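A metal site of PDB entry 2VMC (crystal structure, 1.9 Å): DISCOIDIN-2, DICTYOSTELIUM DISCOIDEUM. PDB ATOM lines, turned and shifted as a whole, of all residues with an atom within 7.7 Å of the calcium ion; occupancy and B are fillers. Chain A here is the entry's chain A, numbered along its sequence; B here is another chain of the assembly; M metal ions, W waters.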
ATOM      1  N   PHE A  37       3.765  16.954  22.717  1.00  0.00           N
ATOM      2  CA  PHE A  37       4.806  16.020  22.281  1.00  0.00           C
ATOM      3  C   PHE A  37       4.369  14.558  22.506  1.00  0.00           C
ATOM      4  O   PHE A  37       3.865  14.205  23.580  1.00  0.00           O
ATOM      5  CB  PHE A  37       6.161  16.250  22.988  1.00  0.00           C
ATOM      6  CG  PHE A  37       7.230  15.243  22.583  1.00  0.00           C
ATOM      7  CD1 PHE A  37       7.943  15.394  21.386  1.00  0.00           C
ATOM      8  CD2 PHE A  37       7.503  14.135  23.380  1.00  0.00           C
ATOM      9  CE1 PHE A  37       8.924  14.432  21.011  1.00  0.00           C
ATOM     10  CE2 PHE A  37       8.473  13.205  23.006  1.00  0.00           C
ATOM     11  CZ  PHE A  37       9.178  13.358  21.820  1.00  0.00           C
ATOM     12  N   SER A  38       4.592  13.732  21.484  1.00  0.00           N
ATOM     13  CA  SER A  38       4.156  12.343  21.481  1.00  0.00           C
ATOM     14  C   SER A  38       5.136  11.543  20.634  1.00  0.00           C
ATOM     15  O   SER A  38       5.502  12.016  19.541  1.00  0.00           O
ATOM     16  CB  SER A  38       2.749  12.273  20.855  1.00  0.00           C
ATOM     17  OG  SER A  38       2.167  10.984  20.969  1.00  0.00           O
ATOM     18  N   ASN A  39       5.528  10.349  21.079  1.00  0.00           N
ATOM     19  CA  ASN A  39       6.381   9.514  20.253  1.00  0.00           C
ATOM     20  C   ASN A  39       5.817   8.080  20.018  1.00  0.00           C
ATOM     21  O   ASN A  39       4.598   7.886  20.089  1.00  0.00           O
ATOM     22  CB  ASN A  39       7.858   9.611  20.688  1.00  0.00           C
ATOM     23  CG  ASN A  39       8.096   9.157  22.132  1.00  0.00           C
ATOM     24  OD1 ASN A  39       7.292   8.408  22.725  1.00  0.00           O
ATOM     25  ND2 ASN A  39       9.250   9.554  22.696  1.00  0.00           N
ATOM     26  N   SER A  40       6.666   7.105  19.699  1.00  0.00           N
ATOM     27  CA  SER A  40       6.170   5.749  19.460  1.00  0.00           C
ATOM     28  C   SER A  40       5.459   5.197  20.719  1.00  0.00           C
ATOM     29  O   SER A  40       5.973   5.304  21.842  1.00  0.00           O
ATOM     30  CB  SER A  40       7.300   4.840  19.012  1.00  0.00           C
ATOM     31  OG  SER A  40       6.812   3.535  18.828  1.00  0.00           O
ATOM     32  N   LYS A  41       4.270   4.637  20.536  1.00  0.00           N
ATOM     33  CA  LYS A  41       3.577   3.984  21.645  1.00  0.00           C
ATOM     34  C   LYS A  41       4.016   2.519  21.770  1.00  0.00           C
ATOM     35  O   LYS A  41       3.288   1.679  22.254  1.00  0.00           O
ATOM     36  CB  LYS A  41       2.051   4.084  21.502  1.00  0.00           C
ATOM     37  CG  LYS A  41       1.538   5.480  21.219  1.00  0.00           C
ATOM     38  CD  LYS A  41       1.762   6.436  22.396  1.00  0.00           C
ATOM     39  CE  LYS A  41       1.896   7.841  21.851  1.00  0.00           C
ATOM     40  NZ  LYS A  41       1.589   8.902  22.838  1.00  0.00           N
ATOM     41  N   ASP A  42       5.218   2.194  21.314  1.00  0.00           N
ATOM     42  CA  ASP A  42       5.810   0.892  21.541  1.00  0.00           C
ATOM     43  C   ASP A  42       6.323   0.746  22.987  1.00  0.00           C
ATOM     44  O   ASP A  42       7.166   1.495  23.445  1.00  0.00           O
ATOM     45  CB  ASP A  42       6.915   0.684  20.504  1.00  0.00           C
ATOM     46  CG  ASP A  42       7.602  -0.656  20.623  1.00  0.00           C
ATOM     47  OD1 ASP A  42       7.323  -1.433  21.573  1.00  0.00           O
ATOM     48  OD2 ASP A  42       8.439  -0.932  19.736  1.00  0.00           O
ATOM     49  N   ALA A  43       5.773  -0.216  23.731  1.00  0.00           N
ATOM     50  CA  ALA A  43       6.156  -0.404  25.115  1.00  0.00           C
ATOM     51  C   ALA A  43       7.444  -1.201  25.287  1.00  0.00           C
ATOM     52  O   ALA A  43       8.019  -1.244  26.389  1.00  0.00           O
ATOM     53  CB  ALA A  43       5.022  -1.083  25.873  1.00  0.00           C
ATOM     54  N   ARG A  45      10.364  -0.767  23.626  1.00  0.00           N
ATOM     55  CA  ARG A  45      11.579  -0.017  23.322  1.00  0.00           C
ATOM     56  C   ARG A  45      11.320   1.419  23.735  1.00  0.00           C
ATOM     57  O   ARG A  45      10.372   2.023  23.245  1.00  0.00           O
ATOM     58  CB  ARG A  45      11.893  -0.042  21.820  1.00  0.00           C
ATOM     59  CG  ARG A  45      13.224   0.626  21.463  1.00  0.00           C
ATOM     60  CD  ARG A  45      13.446   0.658  19.965  1.00  0.00           C
ATOM     61  NE  ARG A  45      12.490   1.506  19.223  1.00  0.00           N
ATOM     62  CZ  ARG A  45      12.518   2.842  19.199  1.00  0.00           C
ATOM     63  NH1 ARG A  45      13.424   3.521  19.907  1.00  0.00           N
ATOM     64  NH2 ARG A  45      11.620   3.477  18.467  1.00  0.00           N
ATOM     65  N   PHE A  46      12.167   1.947  24.611  1.00  0.00           N
ATOM     66  CA  PHE A  46      12.018   3.318  25.125  1.00  0.00           C
ATOM     67  C   PHE A  46      12.685   4.328  24.175  1.00  0.00           C
ATOM     68  O   PHE A  46      13.889   4.231  23.897  1.00  0.00           O
ATOM     69  CB  PHE A  46      12.677   3.411  26.520  1.00  0.00           C
ATOM     70  CG  PHE A  46      12.450   4.714  27.229  1.00  0.00           C
ATOM     71  CD1 PHE A  46      11.161   5.166  27.485  1.00  0.00           C
ATOM     72  CD2 PHE A  46      13.544   5.490  27.673  1.00  0.00           C
ATOM     73  CE1 PHE A  46      10.935   6.394  28.188  1.00  0.00           C
ATOM     74  CE2 PHE A  46      13.328   6.695  28.371  1.00  0.00           C
ATOM     75  CZ  PHE A  46      12.027   7.144  28.619  1.00  0.00           C
ATOM     76  N   ASP A  47      11.894   5.298  23.729  1.00  0.00           N
ATOM     77  CA  ASP A  47      12.363   6.321  22.805  1.00  0.00           C
ATOM     78  C   ASP A  47      12.416   7.721  23.449  1.00  0.00           C
ATOM     79  O   ASP A  47      12.619   8.724  22.755  1.00  0.00           O
ATOM     80  CB  ASP A  47      11.558   6.332  21.471  1.00  0.00           C
ATOM     81  CG  ASP A  47      10.043   6.512  21.662  1.00  0.00           C
ATOM     82  OD1 ASP A  47       9.530   6.466  22.803  1.00  0.00           O
ATOM     83  OD2 ASP A  47       9.345   6.722  20.650  1.00  0.00           O
ATOM     84  N   GLY A  48      12.275   7.765  24.770  1.00  0.00           N
ATOM     85  CA  GLY A  48      12.331   9.022  25.526  1.00  0.00           C
ATOM     86  C   GLY A  48      10.986   9.343  26.166  1.00  0.00           C
ATOM     87  O   GLY A  48       9.925   8.913  25.674  1.00  0.00           O
ATOM     88  N   SER A  49      11.011  10.110  27.267  1.00  0.00           N
ATOM     89  CA  SER A  49       9.776  10.561  27.920  1.00  0.00           C
ATOM     90  C   SER A  49       9.025  11.583  27.044  1.00  0.00           C
ATOM     91  O   SER A  49       9.652  12.360  26.298  1.00  0.00           O
ATOM     92  CB  SER A  49      10.130  11.207  29.279  1.00  0.00           C
ATOM     93  OG  SER A  49      11.032  12.313  29.169  1.00  0.00           O
ATOM     94  N   GLU A  50       7.693  11.578  27.142  1.00  0.00           N
ATOM     95  CA  GLU A  50       6.861  12.645  26.519  1.00  0.00           C
ATOM     96  C   GLU A  50       6.778  13.839  27.469  1.00  0.00           C
ATOM     97  O   GLU A  50       5.694  14.189  27.973  1.00  0.00           O
ATOM     98  CB  GLU A  50       5.470  12.114  26.091  1.00  0.00           C
ATOM     99  CG  GLU A  50       5.591  10.997  25.013  1.00  0.00           C
ATOM    100  CD  GLU A  50       4.276  10.250  24.711  1.00  0.00           C
ATOM    101  OE1 GLU A  50       3.330  10.374  25.518  1.00  0.00           O
ATOM    102  OE2 GLU A  50       4.215   9.568  23.651  1.00  0.00           O
ATOM    103  N   ASP A  83       3.398   9.914  28.847  1.00  0.00           N
ATOM    104  CA  ASP A  83       3.544   8.451  28.920  1.00  0.00           C
ATOM    105  C   ASP A  83       3.701   7.876  30.343  1.00  0.00           C
ATOM    106  O   ASP A  83       3.956   6.663  30.506  1.00  0.00           O
ATOM    107  CB  ASP A  83       4.718   8.020  28.024  1.00  0.00           C
ATOM    108  CG  ASP A  83       6.067   8.576  28.504  1.00  0.00           C
ATOM    109  OD1 ASP A  83       6.185   9.791  28.764  1.00  0.00           O
ATOM    110  OD2 ASP A  83       7.011   7.771  28.614  1.00  0.00           O
ATOM    111  N   SER B  55      11.640   8.302  15.477  1.00  0.00           N
ATOM    112  CA  SER B  55      11.116   7.106  16.148  1.00  0.00           C
ATOM    113  C   SER B  55       9.954   6.458  15.372  1.00  0.00           C
ATOM    114  O   SER B  55       9.978   5.257  15.053  1.00  0.00           O
ATOM    115  CB  SER B  55      10.637   7.440  17.569  1.00  0.00           C
ATOM    116  OG  SER B  55      10.320   6.238  18.264  1.00  0.00           O
HETATM  117 CA    CA M   1       7.290   6.124  23.614  1.00  0.00          CA
HETATM  118  O   HOH W   1       8.342   3.773  23.169  1.00  0.00           O
HETATM  119  O   HOH W   2       6.137   4.414  25.123  1.00  0.00           O
HETATM  120  O   HOH W   3       5.195   7.208  24.449  1.00  0.00           O
HETATM  121  O   HOH W   4       8.305   6.702  25.782  1.00  0.00           O
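Water W4 lies within hydrogen-bond range of the backbone carbonyl oxygen (O) of Gly 48 (2.7 Å) and the side-chain carboxylate (OD2) of Asp 83 (3.3 Å).
OG of Ser 40 lies close to N of Asp 42 (3.2 Å). OG of Ser 55 of chain B is in hydrogen-bond range of OD2 of Asp 47 (2.6 Å). O of Gly 48 is in hydrogen-bond range of ND2 of Asn 39. The backbone NH (N) of Asn 39 sits at hydrogen-bond distance from the side-chain carboxylate (OE2) of Glu 50, at 3.0 Å.
Three residues have an atom within 4 Å of the calcium ion: Asn 39, Ser 40 and Asp 47.
The calcium ion is bound by the backbone carbonyl oxygen of Ser 40 (2.4 Å), the side-chain carboxylate of Asp 47 (2.4 Å), the side-chain amide oxygen of Asn 39 (2.5 Å), water W4 (2.5 Å), water W3 (2.5 Å), water W2 (2.6 Å) and water W1 (2.6 Å). The calcium ion has seven donor atoms within binding distance.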
